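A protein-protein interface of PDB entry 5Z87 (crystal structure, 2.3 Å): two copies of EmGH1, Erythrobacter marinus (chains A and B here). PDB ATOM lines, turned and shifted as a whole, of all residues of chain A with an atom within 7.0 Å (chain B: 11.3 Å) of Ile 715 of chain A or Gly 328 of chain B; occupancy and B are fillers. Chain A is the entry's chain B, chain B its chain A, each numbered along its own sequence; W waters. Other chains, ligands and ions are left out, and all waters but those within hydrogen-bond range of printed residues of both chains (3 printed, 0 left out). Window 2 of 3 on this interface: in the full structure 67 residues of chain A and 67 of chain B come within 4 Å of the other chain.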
ATOM      1  N   ARG A 712      11.010  25.601  42.217  1.00  0.00           N
ATOM      2  CA  ARG A 712      11.337  25.544  40.798  1.00  0.00           C
ATOM      3  C   ARG A 712      12.515  24.601  40.594  1.00  0.00           C
ATOM      4  O   ARG A 712      13.568  24.772  41.218  1.00  0.00           O
ATOM      5  CB  ARG A 712      11.671  26.926  40.218  1.00  0.00           C
ATOM      6  CG  ARG A 712      12.071  26.856  38.746  1.00  0.00           C
ATOM      7  CD  ARG A 712      12.274  28.223  38.115  1.00  0.00           C
ATOM      8  NE  ARG A 712      12.358  28.127  36.657  1.00  0.00           N
ATOM      9  CZ  ARG A 712      12.575  29.162  35.850  1.00  0.00           C
ATOM     10  NH1 ARG A 712      12.734  30.376  36.359  1.00  0.00           N
ATOM     11  NH2 ARG A 712      12.628  28.984  34.537  1.00  0.00           N
ATOM     12  N   ASP A 713      12.331  23.608  39.730  1.00  0.00           N
ATOM     13  CA  ASP A 713      13.413  22.713  39.325  1.00  0.00           C
ATOM     14  C   ASP A 713      14.158  23.371  38.163  1.00  0.00           C
ATOM     15  O   ASP A 713      13.708  23.316  37.015  1.00  0.00           O
ATOM     16  CB  ASP A 713      12.847  21.354  38.934  1.00  0.00           C
ATOM     17  CG  ASP A 713      13.927  20.333  38.609  1.00  0.00           C
ATOM     18  OD1 ASP A 713      15.116  20.622  38.821  1.00  0.00           O
ATOM     19  OD2 ASP A 713      13.582  19.238  38.138  1.00  0.00           O
ATOM     20  N   SER A 714      15.313  23.986  38.453  1.00  0.00           N
ATOM     21  CA  SER A 714      15.920  24.934  37.508  1.00  0.00           C
ATOM     22  C   SER A 714      16.260  24.279  36.176  1.00  0.00           C
ATOM     23  O   SER A 714      16.129  24.901  35.117  1.00  0.00           O
ATOM     24  CB  SER A 714      17.183  25.549  38.106  1.00  0.00           C
ATOM     25  OG  SER A 714      16.860  26.394  39.186  1.00  0.00           O
ATOM     26  N   ILE A 715      16.749  23.048  36.215  1.00  0.00           N
ATOM     27  CA  ILE A 715      17.145  22.301  35.031  1.00  0.00           C
ATOM     28  C   ILE A 715      16.545  20.917  35.180  1.00  0.00           C
ATOM     29  O   ILE A 715      16.602  20.330  36.266  1.00  0.00           O
ATOM     30  CB  ILE A 715      18.679  22.218  34.882  1.00  0.00           C
ATOM     31  CG1 ILE A 715      19.297  23.615  34.781  1.00  0.00           C
ATOM     32  CG2 ILE A 715      19.057  21.376  33.669  1.00  0.00           C
ATOM     33  CD1 ILE A 715      18.992  24.312  33.468  1.00  0.00           C
ATOM     34  N   ALA A 716      15.939  20.411  34.116  1.00  0.00           N
ATOM     35  CA  ALA A 716      15.294  19.116  34.222  1.00  0.00           C
ATOM     36  C   ALA A 716      15.337  18.423  32.874  1.00  0.00           C
ATOM     37  O   ALA A 716      15.503  19.064  31.830  1.00  0.00           O
ATOM     38  CB  ALA A 716      13.856  19.257  34.721  1.00  0.00           C
ATOM     39  N   SER A 717      15.179  17.099  32.899  1.00  0.00           N
ATOM     40  CA  SER A 717      15.264  16.374  31.641  1.00  0.00           C
ATOM     41  C   SER A 717      14.052  16.648  30.760  1.00  0.00           C
ATOM     42  O   SER A 717      14.116  16.407  29.550  1.00  0.00           O
ATOM     43  CB  SER A 717      15.442  14.878  31.893  1.00  0.00           C
ATOM     44  OG  SER A 717      14.450  14.370  32.762  1.00  0.00           O
ATOM     45  N   ARG A 718      12.964  17.163  31.338  1.00  0.00           N
ATOM     46  CA  ARG A 718      11.870  17.784  30.594  1.00  0.00           C
ATOM     47  C   ARG A 718      11.535  19.117  31.244  1.00  0.00           C
ATOM     48  O   ARG A 718      11.605  19.246  32.470  1.00  0.00           O
ATOM     49  CB  ARG A 718      10.633  16.888  30.549  1.00  0.00           C
ATOM     50  CG  ARG A 718      10.871  15.648  29.738  1.00  0.00           C
ATOM     51  CD  ARG A 718       9.601  15.119  29.207  1.00  0.00           C
ATOM     52  NE  ARG A 718       9.800  13.873  28.496  1.00  0.00           N
ATOM     53  CZ  ARG A 718       8.919  13.356  27.645  1.00  0.00           C
ATOM     54  NH1 ARG A 718       7.775  14.002  27.387  1.00  0.00           N
ATOM     55  NH2 ARG A 718       9.186  12.195  27.048  1.00  0.00           N
ATOM     56  N   ARG A 720      10.087  22.104  33.088  1.00  0.00           N
ATOM     57  CA  ARG A 720       9.190  22.092  34.223  1.00  0.00           C
ATOM     58  C   ARG A 720       8.676  23.499  34.507  1.00  0.00           C
ATOM     59  O   ARG A 720       9.270  24.484  34.058  1.00  0.00           O
ATOM     60  CB  ARG A 720       9.914  21.524  35.450  1.00  0.00           C
ATOM     61  CG  ARG A 720      10.129  20.041  35.348  1.00  0.00           C
ATOM     62  CD  ARG A 720      10.725  19.532  36.612  1.00  0.00           C
ATOM     63  NE  ARG A 720       9.792  19.575  37.746  1.00  0.00           N
ATOM     64  CZ  ARG A 720      10.049  19.014  38.927  1.00  0.00           C
ATOM     65  NH1 ARG A 720      11.205  18.378  39.117  1.00  0.00           N
ATOM     66  NH2 ARG A 720       9.164  19.084  39.919  1.00  0.00           N
ATOM     67  N   GLU A 762      16.723  14.337  39.898  1.00  0.00           N
ATOM     68  CA  GLU A 762      17.971  14.560  39.185  1.00  0.00           C
ATOM     69  C   GLU A 762      18.842  15.561  39.926  1.00  0.00           C
ATOM     70  O   GLU A 762      18.322  16.486  40.557  1.00  0.00           O
ATOM     71  CB  GLU A 762      17.693  15.062  37.757  1.00  0.00           C
ATOM     72  CG  GLU A 762      16.576  14.256  37.115  1.00  0.00           C
ATOM     73  CD  GLU A 762      16.059  14.839  35.809  1.00  0.00           C
ATOM     74  OE1 GLU A 762      15.598  14.047  34.969  1.00  0.00           O
ATOM     75  OE2 GLU A 762      16.096  16.072  35.631  1.00  0.00           O
ATOM     76  N   PRO A 763      20.160  15.386  39.899  1.00  0.00           N
ATOM     77  CA  PRO A 763      21.035  16.338  40.586  1.00  0.00           C
ATOM     78  C   PRO A 763      20.875  17.724  39.994  1.00  0.00           C
ATOM     79  O   PRO A 763      20.592  17.883  38.805  1.00  0.00           O
ATOM     80  CB  PRO A 763      22.446  15.781  40.335  1.00  0.00           C
ATOM     81  CG  PRO A 763      22.239  14.330  39.995  1.00  0.00           C
ATOM     82  CD  PRO A 763      20.905  14.270  39.287  1.00  0.00           C
ATOM     83  N   GLY A 764      21.069  18.734  40.832  1.00  0.00           N
ATOM     84  CA  GLY A 764      20.969  20.093  40.346  1.00  0.00           C
ATOM     85  C   GLY A 764      20.234  21.040  41.268  1.00  0.00           C
ATOM     86  O   GLY A 764      19.807  20.672  42.367  1.00  0.00           O
ATOM     87  N   GLU A 765      20.081  22.278  40.817  1.00  0.00           N
ATOM     88  CA  GLU A 765      19.531  23.337  41.647  1.00  0.00           C
ATOM     89  C   GLU A 765      18.011  23.230  41.771  1.00  0.00           C
ATOM     90  O   GLU A 765      17.308  22.942  40.798  1.00  0.00           O
ATOM     91  CB  GLU A 765      19.911  24.692  41.057  1.00  0.00           C
ATOM     92  CG  GLU A 765      19.499  25.881  41.900  1.00  0.00           C
ATOM     93  CD  GLU A 765      19.688  27.178  41.145  1.00  0.00           C
ATOM     94  OE1 GLU A 765      19.009  27.346  40.109  1.00  0.00           O
ATOM     95  OE2 GLU A 765      20.532  28.007  41.565  1.00  0.00           O
ATOM     96  N   ILE A 766      17.513  23.445  42.987  1.00  0.00           N
ATOM     97  CA  ILE A 766      16.099  23.686  43.253  1.00  0.00           C
ATOM     98  C   ILE A 766      15.990  25.061  43.896  1.00  0.00           C
ATOM     99  O   ILE A 766      16.649  25.332  44.908  1.00  0.00           O
ATOM    100  CB  ILE A 766      15.486  22.620  44.175  1.00  0.00           C
ATOM    101  CG1 ILE A 766      15.767  21.209  43.651  1.00  0.00           C
ATOM    102  CG2 ILE A 766      13.973  22.858  44.339  1.00  0.00           C
ATOM    103  CD1 ILE A 766      14.865  20.762  42.507  1.00  0.00           C
ATOM    104  N   GLY B 286       7.078  19.039  27.487  1.00  0.00           N
ATOM    105  CA  GLY B 286       8.386  19.255  28.071  1.00  0.00           C
ATOM    106  C   GLY B 286       9.588  18.960  27.181  1.00  0.00           C
ATOM    107  O   GLY B 286      10.724  19.152  27.630  1.00  0.00           O
ATOM    108  N   PRO B 288      11.774  20.053  24.134  1.00  0.00           N
ATOM    109  CA  PRO B 288      12.050  21.040  23.084  1.00  0.00           C
ATOM    110  C   PRO B 288      12.185  20.353  21.741  1.00  0.00           C
ATOM    111  O   PRO B 288      12.836  19.315  21.629  1.00  0.00           O
ATOM    112  CB  PRO B 288      13.376  21.672  23.531  1.00  0.00           C
ATOM    113  CG  PRO B 288      13.521  21.301  24.994  1.00  0.00           C
ATOM    114  CD  PRO B 288      12.833  19.997  25.151  1.00  0.00           C
ATOM    115  N   ALA B 291      15.458  19.410  20.551  1.00  0.00           N
ATOM    116  CA  ALA B 291      16.031  18.243  21.221  1.00  0.00           C
ATOM    117  C   ALA B 291      15.116  17.026  21.138  1.00  0.00           C
ATOM    118  O   ALA B 291      15.252  16.101  21.941  1.00  0.00           O
ATOM    119  CB  ALA B 291      16.343  18.545  22.690  1.00  0.00           C
ATOM    120  N   VAL B 317      19.286  26.274  19.482  1.00  0.00           N
ATOM    121  CA  VAL B 317      20.050  25.205  20.126  1.00  0.00           C
ATOM    122  C   VAL B 317      20.489  25.649  21.514  1.00  0.00           C
ATOM    123  O   VAL B 317      20.266  24.944  22.503  1.00  0.00           O
ATOM    124  CB  VAL B 317      21.254  24.762  19.265  1.00  0.00           C
ATOM    125  CG1 VAL B 317      21.939  23.575  19.921  1.00  0.00           C
ATOM    126  CG2 VAL B 317      20.812  24.340  17.871  1.00  0.00           C
ATOM    127  N   ARG B 318      21.093  26.838  21.610  1.00  0.00           N
ATOM    128  CA  ARG B 318      21.418  27.413  22.911  1.00  0.00           C
ATOM    129  C   ARG B 318      20.196  27.479  23.830  1.00  0.00           C
ATOM    130  O   ARG B 318      20.311  27.286  25.043  1.00  0.00           O
ATOM    131  CB  ARG B 318      22.004  28.815  22.731  1.00  0.00           C
ATOM    132  CG  ARG B 318      22.493  29.422  24.038  1.00  0.00           C
ATOM    133  CD  ARG B 318      22.780  30.906  23.906  1.00  0.00           C
ATOM    134  NE  ARG B 318      23.282  31.215  22.574  1.00  0.00           N
ATOM    135  CZ  ARG B 318      24.569  31.218  22.246  1.00  0.00           C
ATOM    136  NH1 ARG B 318      25.495  30.941  23.157  1.00  0.00           N
ATOM    137  NH2 ARG B 318      24.923  31.508  21.009  1.00  0.00           N
ATOM    138  N   ARG B 319      19.017  27.755  23.270  1.00  0.00           N
ATOM    139  CA  ARG B 319      17.837  27.958  24.102  1.00  0.00           C
ATOM    140  C   ARG B 319      17.287  26.666  24.683  1.00  0.00           C
ATOM    141  O   ARG B 319      16.436  26.738  25.574  1.00  0.00           O
ATOM    142  CB  ARG B 319      16.750  28.668  23.307  1.00  0.00           C
ATOM    143  CG  ARG B 319      17.032  30.138  23.077  1.00  0.00           C
ATOM    144  CD  ARG B 319      16.097  30.674  22.044  1.00  0.00           C
ATOM    145  NE  ARG B 319      16.521  31.973  21.555  1.00  0.00           N
ATOM    146  CZ  ARG B 319      15.964  32.562  20.505  1.00  0.00           C
ATOM    147  NH1 ARG B 319      14.972  31.954  19.865  1.00  0.00           N
ATOM    148  NH2 ARG B 319      16.395  33.749  20.093  1.00  0.00           N
ATOM    149  N   ILE B 320      17.738  25.501  24.200  1.00  0.00           N
ATOM    150  CA  ILE B 320      17.486  24.252  24.909  1.00  0.00           C
ATOM    151  C   ILE B 320      17.892  24.398  26.363  1.00  0.00           C
ATOM    152  O   ILE B 320      17.242  23.862  27.271  1.00  0.00           O
ATOM    153  CB  ILE B 320      18.246  23.088  24.252  1.00  0.00           C
ATOM    154  CG1 ILE B 320      17.816  22.878  22.798  1.00  0.00           C
ATOM    155  CG2 ILE B 320      18.061  21.790  25.054  1.00  0.00           C
ATOM    156  CD1 ILE B 320      18.791  21.929  22.072  1.00  0.00           C
ATOM    157  N   HIS B 321      18.983  25.121  26.600  1.00  0.00           N
ATOM    158  CA  HIS B 321      19.476  25.426  27.928  1.00  0.00           C
ATOM    159  C   HIS B 321      18.865  26.711  28.472  1.00  0.00           C
ATOM    160  O   HIS B 321      18.258  26.701  29.546  1.00  0.00           O
ATOM    161  CB  HIS B 321      21.003  25.549  27.911  1.00  0.00           C
ATOM    162  CG  HIS B 321      21.559  26.221  29.127  1.00  0.00           C
ATOM    163  ND1 HIS B 321      21.463  25.673  30.390  1.00  0.00           N
ATOM    164  CD2 HIS B 321      22.182  27.415  29.281  1.00  0.00           C
ATOM    165  CE1 HIS B 321      22.020  26.491  31.266  1.00  0.00           C
ATOM    166  NE2 HIS B 321      22.458  27.557  30.621  1.00  0.00           N
ATOM    167  N   SER B 322      18.989  27.808  27.716  1.00  0.00           N
ATOM    168  CA  SER B 322      18.793  29.147  28.265  1.00  0.00           C
ATOM    169  C   SER B 322      17.329  29.569  28.345  1.00  0.00           C
ATOM    170  O   SER B 322      17.016  30.511  29.071  1.00  0.00           O
ATOM    171  CB  SER B 322      19.555  30.175  27.424  1.00  0.00           C
ATOM    172  OG  SER B 322      19.008  30.232  26.110  1.00  0.00           O
ATOM    173  N   LEU B 323      16.441  28.931  27.587  1.00  0.00           N
ATOM    174  CA  LEU B 323      15.017  29.229  27.627  1.00  0.00           C
ATOM    175  C   LEU B 323      14.231  28.097  28.273  1.00  0.00           C
ATOM    176  O   LEU B 323      13.569  28.319  29.287  1.00  0.00           O
ATOM    177  CB  LEU B 323      14.491  29.514  26.211  1.00  0.00           C
ATOM    178  CG  LEU B 323      12.979  29.785  26.151  1.00  0.00           C
ATOM    179  CD1 LEU B 323      12.613  31.035  26.979  1.00  0.00           C
ATOM    180  CD2 LEU B 323      12.521  29.941  24.701  1.00  0.00           C
ATOM    181  N   HIS B 324      14.339  26.874  27.731  1.00  0.00           N
ATOM    182  CA  HIS B 324      13.567  25.734  28.215  1.00  0.00           C
ATOM    183  C   HIS B 324      14.096  25.157  29.528  1.00  0.00           C
ATOM    184  O   HIS B 324      13.337  24.519  30.268  1.00  0.00           O
ATOM    185  CB  HIS B 324      13.561  24.629  27.162  1.00  0.00           C
ATOM    186  CG  HIS B 324      12.771  24.964  25.944  1.00  0.00           C
ATOM    187  ND1 HIS B 324      11.391  24.960  25.932  1.00  0.00           N
ATOM    188  CD2 HIS B 324      13.162  25.316  24.696  1.00  0.00           C
ATOM    189  CE1 HIS B 324      10.967  25.278  24.722  1.00  0.00           C
ATOM    190  NE2 HIS B 324      12.022  25.505  23.955  1.00  0.00           N
ATOM    191  N   GLY B 325      15.381  25.326  29.825  1.00  0.00           N
ATOM    192  CA  GLY B 325      15.907  24.732  31.043  1.00  0.00           C
ATOM    193  C   GLY B 325      16.021  23.227  30.982  1.00  0.00           C
ATOM    194  O   GLY B 325      15.865  22.552  32.004  1.00  0.00           O
ATOM    195  N   VAL B 326      16.287  22.676  29.802  1.00  0.00           N
ATOM    196  CA  VAL B 326      16.420  21.240  29.638  1.00  0.00           C
ATOM    197  C   VAL B 326      17.883  20.817  29.598  1.00  0.00           C
ATOM    198  O   VAL B 326      18.253  19.821  30.219  1.00  0.00           O
ATOM    199  CB  VAL B 326      15.650  20.775  28.385  1.00  0.00           C
ATOM    200  CG1 VAL B 326      16.024  19.333  28.000  1.00  0.00           C
ATOM    201  CG2 VAL B 326      14.153  20.887  28.644  1.00  0.00           C
ATOM    202  N   ALA B 327      18.732  21.579  28.912  1.00  0.00           N
ATOM    203  CA  ALA B 327      20.166  21.349  28.937  1.00  0.00           C
ATOM    204  C   ALA B 327      20.794  22.109  30.099  1.00  0.00           C
ATOM    205  O   ALA B 327      20.440  23.259  30.370  1.00  0.00           O
ATOM    206  CB  ALA B 327      20.809  21.787  27.617  1.00  0.00           C
ATOM    207  N   GLY B 328      21.749  21.462  30.773  1.00  0.00           N
ATOM    208  CA  GLY B 328      22.398  22.072  31.916  1.00  0.00           C
ATOM    209  C   GLY B 328      23.398  23.149  31.565  1.00  0.00           C
ATOM    210  O   GLY B 328      23.763  23.949  32.434  1.00  0.00           O
ATOM    211  N   SER B 329      23.828  23.210  30.310  1.00  0.00           N
ATOM    212  CA  SER B 329      24.815  24.200  29.911  1.00  0.00           C
ATOM    213  C   SER B 329      24.721  24.379  28.404  1.00  0.00           C
ATOM    214  O   SER B 329      24.039  23.625  27.713  1.00  0.00           O
ATOM    215  CB  SER B 329      26.223  23.760  30.313  1.00  0.00           C
ATOM    216  OG  SER B 329      26.513  22.506  29.713  1.00  0.00           O
ATOM    217  N   GLU B 330      25.457  25.365  27.895  1.00  0.00           N
ATOM    218  CA  GLU B 330      25.519  25.553  26.449  1.00  0.00           C
ATOM    219  C   GLU B 330      26.195  24.373  25.760  1.00  0.00           C
ATOM    220  O   GLU B 330      25.729  23.913  24.709  1.00  0.00           O
ATOM    221  CB  GLU B 330      26.228  26.860  26.127  1.00  0.00           C
ATOM    222  CG  GLU B 330      25.579  28.051  26.792  1.00  0.00           C
ATOM    223  CD  GLU B 330      26.143  29.361  26.277  1.00  0.00           C
ATOM    224  OE1 GLU B 330      27.379  29.451  26.133  1.00  0.00           O
ATOM    225  OE2 GLU B 330      25.353  30.294  26.002  1.00  0.00           O
ATOM    226  N   ALA B 331      27.271  23.844  26.349  1.00  0.00           N
ATOM    227  CA  ALA B 331      27.909  22.647  25.799  1.00  0.00           C
ATOM    228  C   ALA B 331      26.949  21.466  25.765  1.00  0.00           C
ATOM    229  O   ALA B 331      26.921  20.709  24.782  1.00  0.00           O
ATOM    230  CB  ALA B 331      29.152  22.282  26.612  1.00  0.00           C
ATOM    231  N   GLU B 332      26.169  21.272  26.843  1.00  0.00           N
ATOM    232  CA  GLU B 332      25.175  20.205  26.825  1.00  0.00           C
ATOM    233  C   GLU B 332      24.088  20.471  25.789  1.00  0.00           C
ATOM    234  O   GLU B 332      23.565  19.527  25.192  1.00  0.00           O
ATOM    235  CB  GLU B 332      24.547  20.003  28.211  1.00  0.00           C
ATOM    236  CG  GLU B 332      23.473  18.906  28.173  1.00  0.00           C
ATOM    237  CD  GLU B 332      22.991  18.402  29.542  1.00  0.00           C
ATOM    238  OE1 GLU B 332      22.744  19.222  30.454  1.00  0.00           O
ATOM    239  OE2 GLU B 332      22.840  17.167  29.692  1.00  0.00           O
ATOM    240  N   ALA B 333      23.752  21.742  25.544  1.00  0.00           N
ATOM    241  CA  ALA B 333      22.740  22.060  24.534  1.00  0.00           C
ATOM    242  C   ALA B 333      23.219  21.683  23.136  1.00  0.00           C
ATOM    243  O   ALA B 333      22.479  21.063  22.357  1.00  0.00           O
ATOM    244  CB  ALA B 333      22.377  23.550  24.591  1.00  0.00           C
ATOM    245  N   ALA B 334      24.455  22.058  22.799  1.00  0.00           N
ATOM    246  CA  ALA B 334      25.026  21.663  21.514  1.00  0.00           C
ATOM    247  C   ALA B 334      24.958  20.153  21.335  1.00  0.00           C
ATOM    248  O   ALA B 334      24.551  19.665  20.273  1.00  0.00           O
ATOM    249  CB  ALA B 334      26.471  22.170  21.410  1.00  0.00           C
ATOM    250  N   ILE B 335      25.284  19.393  22.390  1.00  0.00           N
ATOM    251  CA  ILE B 335      25.303  17.934  22.281  1.00  0.00           C
ATOM    252  C   ILE B 335      23.896  17.389  22.068  1.00  0.00           C
ATOM    253  O   ILE B 335      23.676  16.507  21.227  1.00  0.00           O
ATOM    254  CB  ILE B 335      25.964  17.302  23.518  1.00  0.00           C
ATOM    255  CG1 ILE B 335      27.450  17.648  23.565  1.00  0.00           C
ATOM    256  CG2 ILE B 335      25.788  15.776  23.486  1.00  0.00           C
ATOM    257  CD1 ILE B 335      28.167  17.100  24.801  1.00  0.00           C
ATOM    258  N   MET B 336      22.920  17.893  22.833  1.00  0.00           N
ATOM    259  CA  MET B 336      21.538  17.440  22.668  1.00  0.00           C
ATOM    260  C   MET B 336      21.019  17.718  21.260  1.00  0.00           C
ATOM    261  O   MET B 336      20.444  16.833  20.615  1.00  0.00           O
ATOM    262  CB  MET B 336      20.639  18.106  23.706  1.00  0.00           C
ATOM    263  CG  MET B 336      20.790  17.534  25.096  1.00  0.00           C
ATOM    264  SD  MET B 336      19.622  18.294  26.249  1.00  0.00           S
ATOM    265  CE  MET B 336      20.126  17.500  27.778  1.00  0.00           C
ATOM    266  N   GLY B 337      21.209  18.949  20.763  1.00  0.00           N
ATOM    267  CA  GLY B 337      20.738  19.268  19.421  1.00  0.00           C
ATOM    268  C   GLY B 337      21.370  18.404  18.338  1.00  0.00           C
ATOM    269  O   GLY B 337      20.682  17.910  17.434  1.00  0.00           O
ATOM    270  N   VAL B 351      26.404  27.734  19.832  1.00  0.00           N
ATOM    271  CA  VAL B 351      26.970  26.708  20.694  1.00  0.00           C
ATOM    272  C   VAL B 351      27.639  25.607  19.871  1.00  0.00           C
ATOM    273  O   VAL B 351      28.503  24.891  20.395  1.00  0.00           O
ATOM    274  CB  VAL B 351      25.907  26.137  21.662  1.00  0.00           C
ATOM    275  CG1 VAL B 351      25.326  27.243  22.528  1.00  0.00           C
ATOM    276  CG2 VAL B 351      24.800  25.391  20.911  1.00  0.00           C
ATOM    277  N   MET B 354      31.448  24.965  19.851  1.00  0.00           N
ATOM    278  CA  MET B 354      32.097  24.097  20.828  1.00  0.00           C
ATOM    279  C   MET B 354      32.258  22.663  20.339  1.00  0.00           C
ATOM    280  O   MET B 354      32.925  21.874  21.013  1.00  0.00           O
ATOM    281  CB  MET B 354      31.305  24.073  22.148  1.00  0.00           C
ATOM    282  CG  MET B 354      31.159  25.420  22.846  1.00  0.00           C
ATOM    283  SD  MET B 354      30.016  25.339  24.255  1.00  0.00           S
ATOM    284  CE  MET B 354      29.890  27.078  24.672  1.00  0.00           C
ATOM    285  N   LEU B 358      34.621  19.639  21.973  1.00  0.00           N
ATOM    286  CA  LEU B 358      33.899  18.591  22.698  1.00  0.00           C
ATOM    287  C   LEU B 358      34.297  17.211  22.201  1.00  0.00           C
ATOM    288  O   LEU B 358      34.406  16.267  22.991  1.00  0.00           O
ATOM    289  CB  LEU B 358      32.381  18.781  22.570  1.00  0.00           C
ATOM    290  CG  LEU B 358      31.818  19.984  23.330  1.00  0.00           C
ATOM    291  CD1 LEU B 358      30.469  20.410  22.756  1.00  0.00           C
ATOM    292  CD2 LEU B 358      31.730  19.681  24.836  1.00  0.00           C
HETATM  293  O   HOH W   1      14.393  28.032  31.837  1.00  0.00           O
HETATM  294  O   HOH W   2      12.415  23.696  33.051  1.00  0.00           O
HETATM  295  O   HOH W   3      18.313  17.826  32.134  1.00  0.00           O
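The backbone NH (N) of Ala 716 of chain A is in hydrogen-bond range of the backbone carbonyl oxygen (O) of Gly 325 of chain B, 3.0 Å away. The backbone carbonyl oxygen of Val 326 of chain B lies close to the backbone carbonyl oxygen of Ala 716 of chain A.
O of Ile 320 of chain B is in hydrogen-bond range of N of Gly 325 of chain B (3.5 Å). O of Ile 320 of chain B is in hydrogen-bond range of N of Val 326 of chain B, at 3.0 Å. The backbone carbonyl oxygen of Ile 320 of chain B is in hydrogen-bond range of the backbone NH of Ala 327 of chain B, at 3.2 Å. The backbone carbonyl oxygen (O) of Ala 327 of chain B sits at hydrogen-bond distance from a ring nitrogen (ND1) of His 321 of chain B, 2.6 Å away. N of Gly 328 of chain B sits at hydrogen-bond distance from OE1 of Glu 332 of chain B, 2.5 Å away. The side-chain carboxylate (OE1) of Glu 762 of chain A sits at hydrogen-bond distance from the side-chain hydroxyl (OG) of Ser 717 of chain A (2.5 Å).
Among the printed residues, merely in contact across the chains: Ser 714 of chain A with Gly 325 of chain B (3.9 Å), Ile 715 of chain A with Gly 325 of chain B (3.3 Å), Ile 715 of chain A with Val 326 of chain B (3.9 Å), Ile 715 of chain A with Ala 327 of chain B (3.6 Å), Ile 715 of chain A with Gly 328 of chain B (3.8 Å), Ser 717 of chain A with Val 326 of chain B (3.8 Å) and Arg 718 of chain A with Gly 286 of chain B (3.5 Å).
No residue of chain B comes within 4 Å of Asp 713 of chain A. Ser 714 of chain A touches just one residue of chain B: Gly 325. Of chain B, only Gly 325, Val 326, Ala 327 and Gly 328 come within 4 Å of Ile 715 of chain A. Ala 716 of chain A touches two residues of chain B. Printed residues of chain B within 4 Å of Arg 718 of chain A: Gly 286. Pro 763 of chain A touches none of the printed residues of chain B. No residue of chain B comes within 4 Å of Gly 764 of chain A. Printed residues of chain A within 4 Å of Ala 327 of chain B: Ile 715 (3.6 Å). Of chain A, only Ile 715 (3.8 Å) comes within 4 Å of Gly 328 of chain B. Glu 330 of chain B touches none of the printed residues of chain A. The nearest residue of chain B that does not touch Ile 715 of chain A is His 321 of chain B (4.2 Å). The nearest residue of chain A that does not touch Gly 328 of chain B is Ala 716 of chain A (6.8 Å).
Of the 13 printed residues of chain A, 5 touch a printed residue of chain B. Hydrophobic or aromatic side chains of chain B within 4 Å of the printed part of chain A: Val 326. Along chain B the printed residues that touch a printed residue of chain A span positions 286 to 328. Among the printed residues, 9 pairs touch across the chains.
No position is printed for both chains. Of the 9 pairs that touch across the chains among the printed residues, none has its exchanged pair printed and touching as well.
Water W1 bridges the backbone carbonyl oxygen (O) of Leu 323 of chain B (2.7 Å) and the guanidinium group (NH2) of Arg 712 of chain A (3.4 Å). Water W3 lies within hydrogen-bond range of the backbone carbonyl oxygen (O) of Val 326 of chain B (2.8 Å), the backbone carbonyl oxygen (O) of Ala 716 of chain A (3.1 Å) and the backbone NH (N) of Ser 717 of chain A (3.3 Å). Water W2 lies within hydrogen-bond range of the backbone NH (N) of Arg 720 of chain A (2.8 Å) and the backbone carbonyl oxygen (O) of His 324 of chain B (3.0 Å).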
